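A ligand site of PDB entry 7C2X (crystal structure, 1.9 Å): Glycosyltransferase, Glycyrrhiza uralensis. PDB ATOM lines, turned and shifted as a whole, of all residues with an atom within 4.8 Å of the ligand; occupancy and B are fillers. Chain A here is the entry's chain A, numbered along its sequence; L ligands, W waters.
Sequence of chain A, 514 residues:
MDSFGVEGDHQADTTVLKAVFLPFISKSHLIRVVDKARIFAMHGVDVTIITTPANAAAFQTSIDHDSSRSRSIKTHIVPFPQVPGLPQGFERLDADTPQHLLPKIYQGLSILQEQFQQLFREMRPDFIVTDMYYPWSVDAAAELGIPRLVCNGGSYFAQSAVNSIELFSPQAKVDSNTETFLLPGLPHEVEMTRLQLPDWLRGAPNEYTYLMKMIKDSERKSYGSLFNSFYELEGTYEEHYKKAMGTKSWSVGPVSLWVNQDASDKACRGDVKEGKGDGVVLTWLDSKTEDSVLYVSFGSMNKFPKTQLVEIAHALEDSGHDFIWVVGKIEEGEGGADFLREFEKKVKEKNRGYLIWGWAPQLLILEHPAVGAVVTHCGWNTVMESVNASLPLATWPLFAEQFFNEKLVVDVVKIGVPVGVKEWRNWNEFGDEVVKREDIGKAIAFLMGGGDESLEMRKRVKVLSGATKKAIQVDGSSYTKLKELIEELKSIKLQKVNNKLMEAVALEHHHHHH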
ATOM      1  N   SER A  28     -17.416 -11.900 -16.645  1.00  0.00           N
ATOM      2  CA  SER A  28     -17.527 -13.261 -16.139  1.00  0.00           C
ATOM      3  C   SER A  28     -17.027 -14.297 -17.164  1.00  0.00           C
ATOM      4  O   SER A  28     -16.324 -15.247 -16.801  1.00  0.00           O
ATOM      5  CB  SER A  28     -18.985 -13.532 -15.747  1.00  0.00           C
ATOM      6  OG  SER A  28     -19.246 -14.895 -15.532  1.00  0.00           O
ATOM      7  N   ILE A  31     -13.078 -14.021 -17.472  1.00  0.00           N
ATOM      8  CA  ILE A  31     -12.215 -14.624 -16.465  1.00  0.00           C
ATOM      9  C   ILE A  31     -12.378 -16.139 -16.429  1.00  0.00           C
ATOM     10  O   ILE A  31     -11.415 -16.849 -16.083  1.00  0.00           O
ATOM     11  CB  ILE A  31     -12.401 -13.975 -15.078  1.00  0.00           C
ATOM     12  CG1 ILE A  31     -13.769 -14.270 -14.473  1.00  0.00           C
ATOM     13  CG2 ILE A  31     -12.198 -12.456 -15.161  1.00  0.00           C
ATOM     14  CD1 ILE A  31     -14.095 -13.324 -13.283  1.00  0.00           C
ATOM     15  N   ARG A 269      -7.821 -11.576  -8.982  1.00  0.00           N
ATOM     16  CA  ARG A 269      -8.650 -12.156 -10.032  1.00  0.00           C
ATOM     17  C   ARG A 269      -9.666 -11.158 -10.553  1.00  0.00           C
ATOM     18  O   ARG A 269     -10.490 -10.642  -9.789  1.00  0.00           O
ATOM     19  CB  ARG A 269      -9.366 -13.395  -9.517  1.00  0.00           C
ATOM     20  CG  ARG A 269     -10.144 -14.139 -10.591  1.00  0.00           C
ATOM     21  CD  ARG A 269     -10.349 -15.574 -10.135  1.00  0.00           C
ATOM     22  NE  ARG A 269     -10.835 -16.461 -11.200  1.00  0.00           N
ATOM     23  CZ  ARG A 269     -12.069 -16.935 -11.240  1.00  0.00           C
ATOM     24  NH1 ARG A 269     -12.938 -16.596 -10.291  1.00  0.00           N
ATOM     25  NH2 ARG A 269     -12.426 -17.753 -12.224  1.00  0.00           N
ATOM     26  N   SER A 297     -23.988 -11.160  -3.026  1.00  0.00           N
ATOM     27  CA  SER A 297     -23.501 -10.646  -4.299  1.00  0.00           C
ATOM     28  C   SER A 297     -24.368 -11.181  -5.424  1.00  0.00           C
ATOM     29  O   SER A 297     -24.782 -12.336  -5.403  1.00  0.00           O
ATOM     30  CB  SER A 297     -22.036 -11.049  -4.529  1.00  0.00           C
ATOM     31  OG  SER A 297     -21.561 -10.579  -5.788  1.00  0.00           O
ATOM     32  N   GLY A 299     -23.370 -10.997  -8.795  1.00  0.00           N
ATOM     33  CA  GLY A 299     -22.575 -11.231  -9.980  1.00  0.00           C
ATOM     34  C   GLY A 299     -22.016  -9.958 -10.586  1.00  0.00           C
ATOM     35  O   GLY A 299     -22.035  -8.877  -9.988  1.00  0.00           O
ATOM     36  N   SER A 300     -21.513 -10.097 -11.817  1.00  0.00           N
ATOM     37  CA  SER A 300     -20.796  -9.030 -12.505  1.00  0.00           C
ATOM     38  C   SER A 300     -21.694  -8.149 -13.386  1.00  0.00           C
ATOM     39  O   SER A 300     -21.236  -7.096 -13.836  1.00  0.00           O
ATOM     40  CB  SER A 300     -19.650  -9.607 -13.342  1.00  0.00           C
ATOM     41  OG  SER A 300     -20.132 -10.304 -14.488  1.00  0.00           O
ATOM     42  N   MET A 301     -22.944  -8.548 -13.634  1.00  0.00           N
ATOM     43  CA  MET A 301     -23.789  -7.875 -14.629  1.00  0.00           C
ATOM     44  C   MET A 301     -25.039  -7.222 -14.067  1.00  0.00           C
ATOM     45  O   MET A 301     -25.665  -6.418 -14.777  1.00  0.00           O
ATOM     46  CB  MET A 301     -24.235  -8.871 -15.721  1.00  0.00           C
ATOM     47  CG  MET A 301     -23.088  -9.658 -16.351  1.00  0.00           C
ATOM     48  SD  MET A 301     -21.895  -8.575 -17.177  1.00  0.00           S
ATOM     49  CE  MET A 301     -22.983  -7.609 -18.219  1.00  0.00           C
ATOM     50  N   VAL A 326     -22.108  -6.872  -1.531  1.00  0.00           N
ATOM     51  CA  VAL A 326     -21.493  -6.319  -2.738  1.00  0.00           C
ATOM     52  C   VAL A 326     -22.622  -5.683  -3.531  1.00  0.00           C
ATOM     53  O   VAL A 326     -23.456  -6.388  -4.105  1.00  0.00           O
ATOM     54  CB  VAL A 326     -20.760  -7.386  -3.555  1.00  0.00           C
ATOM     55  CG1 VAL A 326     -20.051  -6.750  -4.779  1.00  0.00           C
ATOM     56  CG2 VAL A 326     -19.750  -8.113  -2.680  1.00  0.00           C
ATOM     57  N   GLY A 358     -17.348  -1.486  -5.214  1.00  0.00           N
ATOM     58  CA  GLY A 358     -16.754  -1.818  -6.483  1.00  0.00           C
ATOM     59  C   GLY A 358     -16.633  -3.314  -6.706  1.00  0.00           C
ATOM     60  O   GLY A 358     -17.522  -4.094  -6.354  1.00  0.00           O
ATOM     61  N   TRP A 359     -15.515  -3.714  -7.304  1.00  0.00           N
ATOM     62  CA  TRP A 359     -15.196  -5.114  -7.545  1.00  0.00           C
ATOM     63  C   TRP A 359     -14.689  -5.740  -6.250  1.00  0.00           C
ATOM     64  O   TRP A 359     -13.664  -5.317  -5.723  1.00  0.00           O
ATOM     65  CB  TRP A 359     -14.139  -5.215  -8.637  1.00  0.00           C
ATOM     66  CG  TRP A 359     -13.805  -6.604  -9.085  1.00  0.00           C
ATOM     67  CD1 TRP A 359     -12.649  -7.291  -8.853  1.00  0.00           C
ATOM     68  CD2 TRP A 359     -14.618  -7.474  -9.889  1.00  0.00           C
ATOM     69  NE1 TRP A 359     -12.693  -8.530  -9.443  1.00  0.00           N
ATOM     70  CE2 TRP A 359     -13.897  -8.672 -10.087  1.00  0.00           C
ATOM     71  CE3 TRP A 359     -15.897  -7.351 -10.449  1.00  0.00           C
ATOM     72  CZ2 TRP A 359     -14.404  -9.749 -10.819  1.00  0.00           C
ATOM     73  CZ3 TRP A 359     -16.407  -8.414 -11.183  1.00  0.00           C
ATOM     74  CH2 TRP A 359     -15.659  -9.604 -11.344  1.00  0.00           C
ATOM     75  N   ALA A 360     -15.423  -6.758  -5.726  1.00  0.00           N
ATOM     76  CA  ALA A 360     -14.974  -7.371  -4.482  1.00  0.00           C
ATOM     77  C   ALA A 360     -14.003  -8.516  -4.764  1.00  0.00           C
ATOM     78  O   ALA A 360     -14.097  -9.176  -5.811  1.00  0.00           O
ATOM     79  CB  ALA A 360     -16.159  -7.903  -3.679  1.00  0.00           C
ATOM     80  N   GLN A 362     -13.794 -11.689  -4.400  1.00  0.00           N
ATOM     81  CA  GLN A 362     -14.769 -12.697  -3.966  1.00  0.00           C
ATOM     82  C   GLN A 362     -14.084 -13.959  -3.453  1.00  0.00           C
ATOM     83  O   GLN A 362     -14.498 -14.520  -2.425  1.00  0.00           O
ATOM     84  CB  GLN A 362     -15.725 -13.035  -5.106  1.00  0.00           C
ATOM     85  CG  GLN A 362     -16.785 -14.048  -4.693  1.00  0.00           C
ATOM     86  CD  GLN A 362     -18.015 -14.012  -5.591  1.00  0.00           C
ATOM     87  OE1 GLN A 362     -18.623 -12.964  -5.789  1.00  0.00           O
ATOM     88  NE2 GLN A 362     -18.385 -15.163  -6.143  1.00  0.00           N
ATOM     89  N   LEU A 363     -13.030 -14.421  -4.120  1.00  0.00           N
ATOM     90  CA  LEU A 363     -12.405 -15.672  -3.684  1.00  0.00           C
ATOM     91  C   LEU A 363     -11.786 -15.523  -2.295  1.00  0.00           C
ATOM     92  O   LEU A 363     -11.874 -16.443  -1.459  1.00  0.00           O
ATOM     93  CB  LEU A 363     -11.363 -16.133  -4.705  1.00  0.00           C
ATOM     94  CG  LEU A 363     -11.859 -16.553  -6.096  1.00  0.00           C
ATOM     95  CD1 LEU A 363     -10.709 -17.137  -6.921  1.00  0.00           C
ATOM     96  CD2 LEU A 363     -12.993 -17.554  -6.001  1.00  0.00           C
ATOM     97  N   HIS A 377     -27.232 -14.767  -7.017  1.00  0.00           N
ATOM     98  CA  HIS A 377     -28.149 -14.842  -8.151  1.00  0.00           C
ATOM     99  C   HIS A 377     -28.021 -16.146  -8.915  1.00  0.00           C
ATOM    100  O   HIS A 377     -28.676 -16.277  -9.963  1.00  0.00           O
ATOM    101  CB  HIS A 377     -27.929 -13.658  -9.113  1.00  0.00           C
ATOM    102  CG  HIS A 377     -26.647 -13.718  -9.875  1.00  0.00           C
ATOM    103  ND1 HIS A 377     -25.434 -14.026  -9.287  1.00  0.00           N
ATOM    104  CD2 HIS A 377     -26.373 -13.511 -11.189  1.00  0.00           C
ATOM    105  CE1 HIS A 377     -24.486 -14.014 -10.206  1.00  0.00           C
ATOM    106  NE2 HIS A 377     -25.031 -13.697 -11.362  1.00  0.00           N
ATOM    107  N   GLY A 379     -25.497 -17.285 -10.526  1.00  0.00           N
ATOM    108  CA  GLY A 379     -24.428 -17.332 -11.509  1.00  0.00           C
ATOM    109  C   GLY A 379     -23.581 -18.563 -11.228  1.00  0.00           C
ATOM    110  O   GLY A 379     -23.244 -18.859 -10.076  1.00  0.00           O
ATOM    111  N   TRP A 380     -23.239 -19.301 -12.279  1.00  0.00           N
ATOM    112  CA  TRP A 380     -22.613 -20.603 -12.057  1.00  0.00           C
ATOM    113  C   TRP A 380     -21.238 -20.467 -11.394  1.00  0.00           C
ATOM    114  O   TRP A 380     -20.843 -21.326 -10.590  1.00  0.00           O
ATOM    115  CB  TRP A 380     -22.492 -21.347 -13.368  1.00  0.00           C
ATOM    116  CG  TRP A 380     -22.097 -22.764 -13.167  1.00  0.00           C
ATOM    117  CD1 TRP A 380     -21.009 -23.394 -13.664  1.00  0.00           C
ATOM    118  CD2 TRP A 380     -22.802 -23.727 -12.379  1.00  0.00           C
ATOM    119  NE1 TRP A 380     -20.983 -24.697 -13.244  1.00  0.00           N
ATOM    120  CE2 TRP A 380     -22.087 -24.932 -12.468  1.00  0.00           C
ATOM    121  CE3 TRP A 380     -23.987 -23.692 -11.636  1.00  0.00           C
ATOM    122  CZ2 TRP A 380     -22.502 -26.085 -11.819  1.00  0.00           C
ATOM    123  CZ3 TRP A 380     -24.393 -24.836 -10.993  1.00  0.00           C
ATOM    124  CH2 TRP A 380     -23.652 -26.022 -11.079  1.00  0.00           C
ATOM    125  N   ASN A 381     -20.489 -19.428 -11.752  1.00  0.00           N
ATOM    126  CA  ASN A 381     -19.181 -19.295 -11.146  1.00  0.00           C
ATOM    127  C   ASN A 381     -19.285 -19.091  -9.631  1.00  0.00           C
ATOM    128  O   ASN A 381     -18.570 -19.735  -8.870  1.00  0.00           O
ATOM    129  CB  ASN A 381     -18.410 -18.174 -11.839  1.00  0.00           C
ATOM    130  CG  ASN A 381     -18.297 -18.412 -13.340  1.00  0.00           C
ATOM    131  OD1 ASN A 381     -17.768 -19.442 -13.766  1.00  0.00           O
ATOM    132  ND2 ASN A 381     -18.858 -17.522 -14.137  1.00  0.00           N
ATOM    133  N   THR A 382     -20.240 -18.270  -9.182  1.00  0.00           N
ATOM    134  CA  THR A 382     -20.390 -18.073  -7.747  1.00  0.00           C
ATOM    135  C   THR A 382     -20.871 -19.345  -7.056  1.00  0.00           C
ATOM    136  O   THR A 382     -20.435 -19.659  -5.944  1.00  0.00           O
ATOM    137  CB  THR A 382     -21.321 -16.891  -7.466  1.00  0.00           C
ATOM    138  OG1 THR A 382     -20.739 -15.705  -8.028  1.00  0.00           O
ATOM    139  CG2 THR A 382     -21.513 -16.669  -5.961  1.00  0.00           C
ATOM    140  N   GLU A 385     -17.758 -21.518  -6.725  1.00  0.00           N
ATOM    141  CA  GLU A 385     -16.830 -20.973  -5.738  1.00  0.00           C
ATOM    142  C   GLU A 385     -17.384 -21.136  -4.330  1.00  0.00           C
ATOM    143  O   GLU A 385     -16.621 -21.424  -3.387  1.00  0.00           O
ATOM    144  CB  GLU A 385     -16.547 -19.513  -6.074  1.00  0.00           C
ATOM    145  CG  GLU A 385     -15.846 -19.330  -7.429  1.00  0.00           C
ATOM    146  CD  GLU A 385     -15.913 -17.891  -7.944  1.00  0.00           C
ATOM    147  OE1 GLU A 385     -16.356 -17.007  -7.176  1.00  0.00           O
ATOM    148  OE2 GLU A 385     -15.535 -17.637  -9.103  1.00  0.00           O
ATOM    149  N   PHE A 399     -31.555 -13.588 -14.405  1.00  0.00           N
ATOM    150  CA  PHE A 399     -31.602 -13.610 -15.858  1.00  0.00           C
ATOM    151  C   PHE A 399     -30.766 -14.777 -16.355  1.00  0.00           C
ATOM    152  O   PHE A 399     -30.419 -15.684 -15.578  1.00  0.00           O
ATOM    153  CB  PHE A 399     -31.128 -12.268 -16.459  1.00  0.00           C
ATOM    154  CG  PHE A 399     -29.855 -11.745 -15.858  1.00  0.00           C
ATOM    155  CD1 PHE A 399     -29.892 -10.912 -14.749  1.00  0.00           C
ATOM    156  CD2 PHE A 399     -28.633 -12.090 -16.401  1.00  0.00           C
ATOM    157  CE1 PHE A 399     -28.708 -10.432 -14.194  1.00  0.00           C
ATOM    158  CE2 PHE A 399     -27.448 -11.611 -15.847  1.00  0.00           C
ATOM    159  CZ  PHE A 399     -27.497 -10.781 -14.744  1.00  0.00           C
ATOM    160  N   GLN A 402     -29.965 -18.603 -14.912  1.00  0.00           N
ATOM    161  CA  GLN A 402     -29.866 -18.694 -13.459  1.00  0.00           C
ATOM    162  C   GLN A 402     -31.048 -19.442 -12.841  1.00  0.00           C
ATOM    163  O   GLN A 402     -30.884 -20.093 -11.801  1.00  0.00           O
ATOM    164  CB  GLN A 402     -29.734 -17.292 -12.863  1.00  0.00           C
ATOM    165  CG  GLN A 402     -28.367 -16.684 -13.144  1.00  0.00           C
ATOM    166  CD  GLN A 402     -28.451 -15.181 -13.341  1.00  0.00           C
ATOM    167  OE1 GLN A 402     -29.344 -14.536 -12.788  1.00  0.00           O
ATOM    168  NE2 GLN A 402     -27.529 -14.628 -14.120  1.00  0.00           N
HETATM  169  N1  LIG L   1     -16.848 -11.520  -8.958  1.00  0.00           N
HETATM  170  C1  LIG L   1     -15.853 -10.941  -8.194  1.00  0.00           C
HETATM  171  N2  LIG L   1     -16.205  -9.761  -7.583  1.00  0.00           N
HETATM  172  C2  LIG L   1     -17.420  -9.112  -7.667  1.00  0.00           C
HETATM  173  C3  LIG L   1     -18.395  -9.778  -8.491  1.00  0.00           C
HETATM  174  C4  LIG L   1     -18.080 -10.923  -9.109  1.00  0.00           C
HETATM  175  O1  LIG L   1     -14.750 -11.436  -8.062  1.00  0.00           O
HETATM  176  O2  LIG L   1     -17.594  -8.046  -7.047  1.00  0.00           O
HETATM  177  C5  LIG L   1     -16.527 -12.752  -9.688  1.00  0.00           C
HETATM  178  C6  LIG L   1     -17.016 -14.026  -9.013  1.00  0.00           C
HETATM  179  O3  LIG L   1     -15.986 -14.558  -8.189  1.00  0.00           O
HETATM  180  C7  LIG L   1     -17.303 -14.919 -10.223  1.00  0.00           C
HETATM  181  C8  LIG L   1     -17.811 -13.934 -11.260  1.00  0.00           C
HETATM  182  O4  LIG L   1     -17.206 -12.664 -10.932  1.00  0.00           O
HETATM  183  O5  LIG L   1     -16.117 -15.542 -10.692  1.00  0.00           O
HETATM  184  C9  LIG L   1     -19.302 -13.762 -11.343  1.00  0.00           C
HETATM  185  O6  LIG L   1     -19.753 -14.801 -12.215  1.00  0.00           O
HETATM  186  P1  LIG L   1     -21.147 -15.514 -12.007  1.00  0.00           P
HETATM  187  O7  LIG L   1     -21.306 -15.745 -10.557  1.00  0.00           O
HETATM  188  O8  LIG L   1     -21.266 -16.747 -12.895  1.00  0.00           O
HETATM  189  O9  LIG L   1     -22.238 -14.429 -12.519  1.00  0.00           O
HETATM  190  P2  LIG L   1     -22.395 -13.445 -13.759  1.00  0.00           P
HETATM  191  O10 LIG L   1     -21.941 -14.293 -14.958  1.00  0.00           O
HETATM  192  O11 LIG L   1     -21.394 -12.333 -13.446  1.00  0.00           O
HETATM  193  O12 LIG L   1     -23.810 -12.950 -13.905  1.00  0.00           O
HETATM  194  O   HOH W   1     -13.335 -14.266  -8.688  1.00  0.00           O
HETATM  195  O   HOH W   2     -24.628 -10.543 -12.627  1.00  0.00           O
HETATM  196  O   HOH W   3     -22.514 -16.625 -15.148  1.00  0.00           O
HETATM  197  O   HOH W   4     -19.453  -6.076  -8.238  1.00  0.00           O
HETATM  198  O   HOH W   5     -22.118 -14.098 -17.751  1.00  0.00           O
HETATM  199  O   HOH W   6     -12.043 -11.252  -7.614  1.00  0.00           O
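OG1 of Thr 382 is in hydrogen-bond range of NE2 of Gln 362.
The side-chain hydroxyl (OG) of Ser 300 sits close to the side-chain sulfur (SD) of Met 301 (3.7 Å).
OE1 of Glu 385 lies within hydrogen-bond range of NE2 of Gln 362 (2.9 Å).
NH1 of Arg 269 lies within salt-bridge range of OE2 of Glu 385 (3.0 Å).
The side-chain hydroxyl (OG) of Ser 28 lies within hydrogen-bond range of the side-chain amide nitrogen (ND2) of Asn 381 (3.0 Å).
ND1 of His 377 sits close to N of Gly 379 (3.5 Å).
The backbone carbonyl oxygen (O) of His 377 sits close to the side-chain amide oxygen (OE1) of Gln 402, 3.4 Å away.
The indole nitrogen (NE1) of Trp 359 sits at hydrogen-bond distance from the backbone carbonyl oxygen (O) of Arg 269.
O7 of the ligand lies within hydrogen-bond range of N of Thr 382.
The side-chain hydroxyl of Thr 382 lies within hydrogen-bond range of an oxygen (O7) of the ligand (2.6 Å).
N of Ser 300 sits at hydrogen-bond distance from O11 of the ligand, 2.8 Å away.
OG of Ser 300 sits at hydrogen-bond distance from O11 of the ligand (2.6 Å).
O3 of the ligand is in hydrogen-bond range of OE1 of Glu 385 (2.7 Å).
N of Ala 360 lies within hydrogen-bond range of O2 of the ligand, at 2.8 Å.
N2 of the ligand lies within hydrogen-bond range of O of Ala 360, at 2.8 Å.
The backbone NH of Asn 381 sits at hydrogen-bond distance from an oxygen (O8) of the ligand (3.0 Å).
ND2 of Asn 381 lies within hydrogen-bond range of O8 of the ligand (2.8 Å).
OG of Ser 28 sits at hydrogen-bond distance from O10 of the ligand, at 2.8 Å.
A ring nitrogen (NE2) of His 377 lies within hydrogen-bond range of an oxygen (O12) of the ligand, at 2.9 Å.
NE2 of Gln 362 lies within hydrogen-bond range of O3 of the ligand, 3.2 Å away.
An oxygen (O8) of the ligand sits at hydrogen-bond distance from the backbone NH of Trp 380.
O5 of the ligand is in hydrogen-bond range of NH1 of Arg 269.
Ile 31 touches the ligand (CD1 to O4, 3.95 Å).
C of Gly 299 touches O11 of the ligand (3.8 Å).
Val 326 touches the ligand (CG1 to O2, 3.6 Å).
Trp 359 touches the ligand (CZ2 to C1, 3.2 Å).
C of Gly 379 touches O8 of the ligand, 3.4 Å away.
Of the 21 residues printed, 15 come within 4 Å of the ligand.
The nearest printed residue that does not touch the ligand is Gly 358 (4.01 Å).
Water W1 lies within hydrogen-bond range of O3 of the ligand (2.7 Å) and NH1 of Arg 269 (2.9 Å).
Water W2 lies within hydrogen-bond range of N of Met 301, O12 of the ligand, N of Ser 300 and NE2 of His 377.
Water W4 lies within hydrogen-bond range of an oxygen (O2) of the ligand (3.0 Å) and the backbone carbonyl oxygen of Gly 358 (3.3 Å).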
